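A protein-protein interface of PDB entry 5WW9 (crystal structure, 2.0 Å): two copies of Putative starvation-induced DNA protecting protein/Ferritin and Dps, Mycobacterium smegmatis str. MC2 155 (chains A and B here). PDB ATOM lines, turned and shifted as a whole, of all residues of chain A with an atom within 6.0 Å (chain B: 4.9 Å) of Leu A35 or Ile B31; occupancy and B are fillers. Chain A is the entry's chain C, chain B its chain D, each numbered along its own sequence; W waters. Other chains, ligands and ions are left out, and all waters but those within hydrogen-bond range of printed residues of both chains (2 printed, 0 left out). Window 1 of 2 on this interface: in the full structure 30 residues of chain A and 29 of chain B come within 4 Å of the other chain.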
ATOM      1  N   LEU A  30      -3.786 -16.308   5.074  1.00  0.00           N
ATOM      2  CA  LEU A  30      -4.279 -16.340   3.690  1.00  0.00           C
ATOM      3  C   LEU A  30      -4.291 -14.944   3.053  1.00  0.00           C
ATOM      4  O   LEU A  30      -3.890 -14.770   1.886  1.00  0.00           O
ATOM      5  CB  LEU A  30      -5.663 -16.986   3.612  1.00  0.00           C
ATOM      6  CG  LEU A  30      -5.740 -18.504   3.831  1.00  0.00           C
ATOM      7  CD1 LEU A  30      -7.200 -18.902   4.015  1.00  0.00           C
ATOM      8  CD2 LEU A  30      -5.100 -19.281   2.684  1.00  0.00           C
ATOM      9  N   ILE A  31      -4.727 -13.955   3.830  1.00  0.00           N
ATOM     10  CA  ILE A  31      -4.760 -12.560   3.364  1.00  0.00           C
ATOM     11  C   ILE A  31      -3.341 -12.036   3.135  1.00  0.00           C
ATOM     12  O   ILE A  31      -3.046 -11.473   2.070  1.00  0.00           O
ATOM     13  CB  ILE A  31      -5.566 -11.636   4.313  1.00  0.00           C
ATOM     14  CG1 ILE A  31      -7.048 -12.029   4.299  1.00  0.00           C
ATOM     15  CG2 ILE A  31      -5.396 -10.178   3.901  1.00  0.00           C
ATOM     16  CD1 ILE A  31      -7.892 -11.344   5.361  1.00  0.00           C
ATOM     17  N   GLU A  32      -2.472 -12.248   4.124  1.00  0.00           N
ATOM     18  CA  GLU A  32      -1.066 -11.867   4.007  1.00  0.00           C
ATOM     19  C   GLU A  32      -0.399 -12.540   2.801  1.00  0.00           C
ATOM     20  O   GLU A  32       0.345 -11.891   2.060  1.00  0.00           O
ATOM     21  CB  GLU A  32      -0.305 -12.158   5.306  1.00  0.00           C
ATOM     22  CG  GLU A  32       1.197 -11.854   5.277  1.00  0.00           C
ATOM     23  CD  GLU A  32       1.550 -10.373   5.128  1.00  0.00           C
ATOM     24  OE1 GLU A  32       0.651  -9.496   5.098  1.00  0.00           O
ATOM     25  OE2 GLU A  32       2.753 -10.085   5.027  1.00  0.00           O
ATOM     26  N   LEU A  33      -0.687 -13.826   2.601  1.00  0.00           N
ATOM     27  CA  LEU A  33      -0.159 -14.554   1.444  1.00  0.00           C
ATOM     28  C   LEU A  33      -0.655 -13.942   0.133  1.00  0.00           C
ATOM     29  O   LEU A  33       0.119 -13.828  -0.828  1.00  0.00           O
ATOM     30  CB  LEU A  33      -0.492 -16.060   1.521  1.00  0.00           C
ATOM     31  CG  LEU A  33       0.088 -16.979   0.430  1.00  0.00           C
ATOM     32  CD1 LEU A  33       1.616 -16.913   0.368  1.00  0.00           C
ATOM     33  CD2 LEU A  33      -0.393 -18.410   0.625  1.00  0.00           C
ATOM     34  N   SER A  34      -1.928 -13.532   0.107  1.00  0.00           N
ATOM     35  CA  SER A  34      -2.510 -12.848  -1.062  1.00  0.00           C
ATOM     36  C   SER A  34      -1.784 -11.538  -1.356  1.00  0.00           C
ATOM     37  O   SER A  34      -1.453 -11.257  -2.509  1.00  0.00           O
ATOM     38  CB  SER A  34      -4.002 -12.565  -0.873  1.00  0.00           C
ATOM     39  OG  SER A  34      -4.730 -13.760  -0.652  1.00  0.00           O
ATOM     40  N   LEU A  35      -1.519 -10.754  -0.313  1.00  0.00           N
ATOM     41  CA  LEU A  35      -0.861  -9.449  -0.489  1.00  0.00           C
ATOM     42  C   LEU A  35       0.603  -9.619  -0.902  1.00  0.00           C
ATOM     43  O   LEU A  35       1.102  -8.878  -1.756  1.00  0.00           O
ATOM     44  CB  LEU A  35      -0.995  -8.583   0.772  1.00  0.00           C
ATOM     45  CG  LEU A  35      -2.409  -8.116   1.156  1.00  0.00           C
ATOM     46  CD1 LEU A  35      -2.406  -7.519   2.556  1.00  0.00           C
ATOM     47  CD2 LEU A  35      -2.987  -7.120   0.151  1.00  0.00           C
ATOM     48  N   GLN A  36       1.272 -10.612  -0.313  1.00  0.00           N
ATOM     49  CA  GLN A  36       2.666 -10.914  -0.658  1.00  0.00           C
ATOM     50  C   GLN A  36       2.794 -11.490  -2.066  1.00  0.00           C
ATOM     51  O   GLN A  36       3.759 -11.199  -2.770  1.00  0.00           O
ATOM     52  CB  GLN A  36       3.292 -11.871   0.350  1.00  0.00           C
ATOM     53  CG  GLN A  36       3.550 -11.263   1.725  1.00  0.00           C
ATOM     54  CD  GLN A  36       4.560 -12.049   2.545  1.00  0.00           C
ATOM     55  OE1 GLN A  36       5.419 -12.736   1.993  1.00  0.00           O
ATOM     56  NE2 GLN A  36       4.489 -11.918   3.870  1.00  0.00           N
ATOM     57  N   GLY A  37       1.821 -12.321  -2.449  1.00  0.00           N
ATOM     58  CA  GLY A  37       1.735 -12.900  -3.790  1.00  0.00           C
ATOM     59  C   GLY A  37       1.628 -11.834  -4.864  1.00  0.00           C
ATOM     60  O   GLY A  37       2.306 -11.918  -5.882  1.00  0.00           O
ATOM     61  N   LYS A  38       0.779 -10.833  -4.634  1.00  0.00           N
ATOM     62  CA  LYS A  38       0.659  -9.714  -5.572  1.00  0.00           C
ATOM     63  C   LYS A  38       1.949  -8.882  -5.627  1.00  0.00           C
ATOM     64  O   LYS A  38       2.401  -8.526  -6.714  1.00  0.00           O
ATOM     65  CB  LYS A  38      -0.571  -8.854  -5.268  1.00  0.00           C
ATOM     66  CG  LYS A  38      -1.831  -9.328  -5.991  1.00  0.00           C
ATOM     67  CD  LYS A  38      -1.762  -9.042  -7.491  1.00  0.00           C
ATOM     68  CE  LYS A  38      -3.000  -9.545  -8.209  1.00  0.00           C
ATOM     69  NZ  LYS A  38      -2.864  -9.347  -9.679  1.00  0.00           N
ATOM     70  N   GLN A  39       2.558  -8.633  -4.463  1.00  0.00           N
ATOM     71  CA  GLN A  39       3.847  -7.913  -4.397  1.00  0.00           C
ATOM     72  C   GLN A  39       4.890  -8.602  -5.282  1.00  0.00           C
ATOM     73  O   GLN A  39       5.530  -7.948  -6.108  1.00  0.00           O
ATOM     74  CB  GLN A  39       4.343  -7.788  -2.944  1.00  0.00           C
ATOM     75  CG  GLN A  39       5.621  -6.974  -2.757  1.00  0.00           C
ATOM     76  CD  GLN A  39       5.450  -5.466  -2.909  1.00  0.00           C
ATOM     77  OE1 GLN A  39       4.338  -4.946  -3.036  1.00  0.00           O
ATOM     78  NE2 GLN A  39       6.572  -4.753  -2.903  1.00  0.00           N
ATOM     79  N   ALA A  40       5.007  -9.922  -5.122  1.00  0.00           N
ATOM     80  CA  ALA A  40       5.931 -10.768  -5.880  1.00  0.00           C
ATOM     81  C   ALA A  40       5.586 -10.806  -7.372  1.00  0.00           C
ATOM     82  O   ALA A  40       6.479 -10.717  -8.220  1.00  0.00           O
ATOM     83  CB  ALA A  40       5.940 -12.175  -5.300  1.00  0.00           C
ATOM     84  N   TRP A  42       4.108  -8.444  -9.131  1.00  0.00           N
ATOM     85  CA  TRP A  42       4.486  -7.180  -9.779  1.00  0.00           C
ATOM     86  C   TRP A  42       5.994  -7.003  -9.913  1.00  0.00           C
ATOM     87  O   TRP A  42       6.463  -6.510 -10.940  1.00  0.00           O
ATOM     88  CB  TRP A  42       3.914  -5.961  -9.046  1.00  0.00           C
ATOM     89  CG  TRP A  42       2.412  -5.937  -8.851  1.00  0.00           C
ATOM     90  CD1 TRP A  42       1.437  -6.261  -9.768  1.00  0.00           C
ATOM     91  CD2 TRP A  42       1.727  -5.538  -7.663  1.00  0.00           C
ATOM     92  NE1 TRP A  42       0.185  -6.097  -9.208  1.00  0.00           N
ATOM     93  CE2 TRP A  42       0.334  -5.656  -7.919  1.00  0.00           C
ATOM     94  CE3 TRP A  42       2.152  -5.087  -6.402  1.00  0.00           C
ATOM     95  CZ2 TRP A  42      -0.635  -5.339  -6.958  1.00  0.00           C
ATOM     96  CZ3 TRP A  42       1.187  -4.775  -5.442  1.00  0.00           C
ATOM     97  CH2 TRP A  42      -0.195  -4.908  -5.729  1.00  0.00           C
ATOM     98  N   VAL A  60      -2.440 -16.118  -5.892  1.00  0.00           N
ATOM     99  CA  VAL A  60      -3.262 -15.031  -5.340  1.00  0.00           C
ATOM    100  C   VAL A  60      -4.758 -15.333  -5.472  1.00  0.00           C
ATOM    101  O   VAL A  60      -5.494 -15.176  -4.504  1.00  0.00           O
ATOM    102  CB  VAL A  60      -2.924 -13.647  -5.938  1.00  0.00           C
ATOM    103  CG1 VAL A  60      -3.841 -12.568  -5.368  1.00  0.00           C
ATOM    104  CG2 VAL A  60      -1.487 -13.271  -5.620  1.00  0.00           C
ATOM    105  N   VAL A  88      -3.918  -7.849  10.119  1.00  0.00           N
ATOM    106  CA  VAL A  88      -3.122  -8.753   9.292  1.00  0.00           C
ATOM    107  C   VAL A  88      -1.614  -8.533   9.544  1.00  0.00           C
ATOM    108  O   VAL A  88      -0.889  -9.483   9.855  1.00  0.00           O
ATOM    109  CB  VAL A  88      -3.523  -8.616   7.797  1.00  0.00           C
ATOM    110  CG1 VAL A  88      -2.494  -9.251   6.871  1.00  0.00           C
ATOM    111  CG2 VAL A  88      -4.902  -9.236   7.565  1.00  0.00           C
ATOM    112  N   LEU B  27      -2.222   3.519  -4.960  1.00  0.00           N
ATOM    113  CA  LEU B  27      -2.132   2.072  -4.752  1.00  0.00           C
ATOM    114  C   LEU B  27      -2.551   1.629  -3.352  1.00  0.00           C
ATOM    115  O   LEU B  27      -3.387   0.735  -3.227  1.00  0.00           O
ATOM    116  CB  LEU B  27      -0.725   1.545  -5.084  1.00  0.00           C
ATOM    117  CG  LEU B  27      -0.478   0.037  -4.860  1.00  0.00           C
ATOM    118  CD1 LEU B  27      -1.230  -0.826  -5.869  1.00  0.00           C
ATOM    119  CD2 LEU B  27       1.006  -0.297  -4.863  1.00  0.00           C
ATOM    120  N   VAL B  28      -1.991   2.260  -2.314  1.00  0.00           N
ATOM    121  CA  VAL B  28      -2.282   1.850  -0.931  1.00  0.00           C
ATOM    122  C   VAL B  28      -3.735   2.085  -0.533  1.00  0.00           C
ATOM    123  O   VAL B  28      -4.298   1.282   0.201  1.00  0.00           O
ATOM    124  CB  VAL B  28      -1.312   2.434   0.141  1.00  0.00           C
ATOM    125  CG1 VAL B  28       0.060   1.792   0.026  1.00  0.00           C
ATOM    126  CG2 VAL B  28      -1.222   3.958   0.068  1.00  0.00           C
ATOM    127  N   ASP B  29      -4.332   3.172  -1.033  1.00  0.00           N
ATOM    128  CA  ASP B  29      -5.730   3.488  -0.716  1.00  0.00           C
ATOM    129  C   ASP B  29      -6.707   2.555  -1.414  1.00  0.00           C
ATOM    130  O   ASP B  29      -7.751   2.226  -0.854  1.00  0.00           O
ATOM    131  CB  ASP B  29      -6.050   4.951  -0.996  1.00  0.00           C
ATOM    132  CG  ASP B  29      -5.507   5.873   0.083  1.00  0.00           C
ATOM    133  OD1 ASP B  29      -5.058   5.383   1.137  1.00  0.00           O
ATOM    134  OD2 ASP B  29      -5.529   7.094  -0.116  1.00  0.00           O
ATOM    135  N   LEU B  30      -6.345   2.111  -2.615  1.00  0.00           N
ATOM    136  CA  LEU B  30      -7.117   1.097  -3.333  1.00  0.00           C
ATOM    137  C   LEU B  30      -7.057  -0.283  -2.651  1.00  0.00           C
ATOM    138  O   LEU B  30      -8.091  -0.956  -2.523  1.00  0.00           O
ATOM    139  CB  LEU B  30      -6.656   1.004  -4.793  1.00  0.00           C
ATOM    140  CG  LEU B  30      -7.117   2.095  -5.768  1.00  0.00           C
ATOM    141  CD1 LEU B  30      -6.362   1.964  -7.082  1.00  0.00           C
ATOM    142  CD2 LEU B  30      -8.617   2.048  -6.017  1.00  0.00           C
ATOM    143  N   ILE B  31      -5.855  -0.699  -2.230  1.00  0.00           N
ATOM    144  CA  ILE B  31      -5.679  -1.945  -1.469  1.00  0.00           C
ATOM    145  C   ILE B  31      -6.419  -1.912  -0.126  1.00  0.00           C
ATOM    146  O   ILE B  31      -7.131  -2.875   0.230  1.00  0.00           O
ATOM    147  CB  ILE B  31      -4.182  -2.312  -1.271  1.00  0.00           C
ATOM    148  CG1 ILE B  31      -3.520  -2.583  -2.622  1.00  0.00           C
ATOM    149  CG2 ILE B  31      -4.027  -3.540  -0.367  1.00  0.00           C
ATOM    150  CD1 ILE B  31      -2.011  -2.657  -2.562  1.00  0.00           C
ATOM    151  N   GLU B  32      -6.248  -0.813   0.614  1.00  0.00           N
ATOM    152  CA  GLU B  32      -6.968  -0.615   1.866  1.00  0.00           C
ATOM    153  C   GLU B  32      -8.486  -0.651   1.653  1.00  0.00           C
ATOM    154  O   GLU B  32      -9.203  -1.268   2.443  1.00  0.00           O
ATOM    155  CB  GLU B  32      -6.534   0.679   2.566  1.00  0.00           C
ATOM    156  CG  GLU B  32      -7.279   0.987   3.871  1.00  0.00           C
ATOM    157  CD  GLU B  32      -6.960   0.040   5.013  1.00  0.00           C
ATOM    158  OE1 GLU B  32      -7.508   0.252   6.112  1.00  0.00           O
ATOM    159  OE2 GLU B  32      -6.169  -0.913   4.833  1.00  0.00           O
ATOM    160  N   LEU B  33      -8.961  -0.010   0.583  1.00  0.00           N
ATOM    161  CA  LEU B  33     -10.386  -0.037   0.248  1.00  0.00           C
ATOM    162  C   LEU B  33     -10.873  -1.456  -0.028  1.00  0.00           C
ATOM    163  O   LEU B  33     -11.969  -1.823   0.398  1.00  0.00           O
ATOM    164  CB  LEU B  33     -10.716   0.898  -0.923  1.00  0.00           C
ATOM    165  CG  LEU B  33     -12.188   1.134  -1.303  1.00  0.00           C
ATOM    166  CD1 LEU B  33     -12.984   1.824  -0.192  1.00  0.00           C
ATOM    167  CD2 LEU B  33     -12.244   1.956  -2.579  1.00  0.00           C
ATOM    168  N   SER B  34     -10.039  -2.236  -0.721  1.00  0.00           N
ATOM    169  CA  SER B  34     -10.318  -3.643  -1.036  1.00  0.00           C
ATOM    170  C   SER B  34     -10.453  -4.482   0.233  1.00  0.00           C
ATOM    171  O   SER B  34     -11.376  -5.288   0.341  1.00  0.00           O
ATOM    172  CB  SER B  34      -9.215  -4.224  -1.927  1.00  0.00           C
ATOM    173  OG  SER B  34      -9.172  -3.561  -3.177  1.00  0.00           O
ATOM    174  N   LEU B  35      -9.532  -4.289   1.181  1.00  0.00           N
ATOM    175  CA  LEU B  35      -9.563  -5.003   2.466  1.00  0.00           C
ATOM    176  C   LEU B  35     -10.757  -4.590   3.338  1.00  0.00           C
ATOM    177  O   LEU B  35     -11.408  -5.431   3.948  1.00  0.00           O
ATOM    178  CB  LEU B  35      -8.233  -4.832   3.224  1.00  0.00           C
ATOM    179  CG  LEU B  35      -6.968  -5.423   2.596  1.00  0.00           C
ATOM    180  CD1 LEU B  35      -5.717  -4.742   3.124  1.00  0.00           C
ATOM    181  CD2 LEU B  35      -6.884  -6.928   2.817  1.00  0.00           C
ATOM    182  N   SER B  67      -6.011  -1.515  -8.279  1.00  0.00           N
ATOM    183  CA  SER B  67      -4.692  -1.621  -7.646  1.00  0.00           C
ATOM    184  C   SER B  67      -3.697  -2.348  -8.554  1.00  0.00           C
ATOM    185  O   SER B  67      -2.560  -1.892  -8.732  1.00  0.00           O
ATOM    186  CB  SER B  67      -4.779  -2.279  -6.258  1.00  0.00           C
ATOM    187  OG  SER B  67      -5.371  -3.564  -6.321  1.00  0.00           O
ATOM    188  N   GLY B  83       2.754  -2.898  -2.063  1.00  0.00           N
ATOM    189  CA  GLY B  83       1.396  -3.218  -1.631  1.00  0.00           C
ATOM    190  C   GLY B  83       1.335  -4.151  -0.432  1.00  0.00           C
ATOM    191  O   GLY B  83       0.330  -4.825  -0.231  1.00  0.00           O
ATOM    192  N   SER B  85       1.137  -5.463   3.522  1.00  0.00           N
ATOM    193  CA  SER B  85       0.179  -5.110   4.590  1.00  0.00           C
ATOM    194  C   SER B  85       0.671  -3.998   5.528  1.00  0.00           C
ATOM    195  O   SER B  85      -0.072  -3.060   5.820  1.00  0.00           O
ATOM    196  CB  SER B  85      -0.222  -6.345   5.398  1.00  0.00           C
ATOM    197  OG  SER B  85       0.921  -6.996   5.906  1.00  0.00           O
ATOM    198  N   VAL B  88       0.612  -0.590   3.575  1.00  0.00           N
ATOM    199  CA  VAL B  88      -0.787  -0.188   3.415  1.00  0.00           C
ATOM    200  C   VAL B  88      -1.339   0.411   4.726  1.00  0.00           C
ATOM    201  O   VAL B  88      -1.868   1.518   4.714  1.00  0.00           O
ATOM    202  CB  VAL B  88      -1.653  -1.364   2.875  1.00  0.00           C
ATOM    203  CG1 VAL B  88      -3.147  -1.044   2.922  1.00  0.00           C
ATOM    204  CG2 VAL B  88      -1.249  -1.701   1.442  1.00  0.00           C
HETATM  205  O   HOH W   1       2.024  -8.143   2.697  1.00  0.00           O
HETATM  206  O   HOH W   2      -0.377  -6.415  -2.388  1.00  0.00           O
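The side-chain carboxylate of Glu A32 is in hydrogen-bond range of the side-chain hydroxyl of Ser B85 (2.6 Å). The backbone NH (N) of Gly B83 sits at hydrogen-bond distance from the side-chain amide oxygen (OE1) of Gln A39 (2.8 Å).
The side-chain carboxylate (OE2) of Glu A32 lies within hydrogen-bond range of the side-chain amide nitrogen (NE2) of Gln A36 (2.8 Å).
Among the printed residues, pairs that only touch across the chains: Ile A31 with Leu B35 (3.7 Å), Leu A35 with Ile B31 (3.8 Å), Leu A35 with Ser B85 (3.8 Å) and Val A88 with Ser B85 (3.97 Å).
Of the printed residues of chain B, Ile A31 touches Leu B35 (3.7 Å). Leu A33 touches none of the printed residues of chain B. Of chain B, only Ile B31 and Ser B85 come within 4 Å of Leu A35. Printed residues of chain A within 4 Å of Ile B31: Leu A35. Of the printed residues of chain A, Leu B35 touches Ile A31 (3.7 Å). The nearest residue of chain A that does not touch Ile B31 is Trp A42 (4.3 Å). The nearest printed residue of chain A that does not touch Ser B85 is Gln A36 (6.4 Å).
Of the 13 printed residues of chain B, 4 touch a printed residue of chain A. Printed residues of chain B that touch a printed residue of chain A: Ile B31, Leu B35, Gly B83 and Ser B85. Hydrophobic or aromatic side chains of chain B within 4 Å of the printed part of chain A: Ile B31 and Leu B35. Among the printed residues, 6 pairs touch across the chains.
Ile A31 touches Leu B35, and with the chains exchanged Leu A35 touches Ile B31. 7 positions are printed for both chains. Of the 6 pairs that touch across the chains among the printed residues, 2 have their exchanged pair printed and touching as well.
Water W2 bridges O of Gly B83 (2.8 Å) and O of Leu A35 (2.9 Å). Water W1 lies within hydrogen-bond range of N of Ser B85 (2.9 Å) and OE1 of Glu A32 (3.1 Å).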
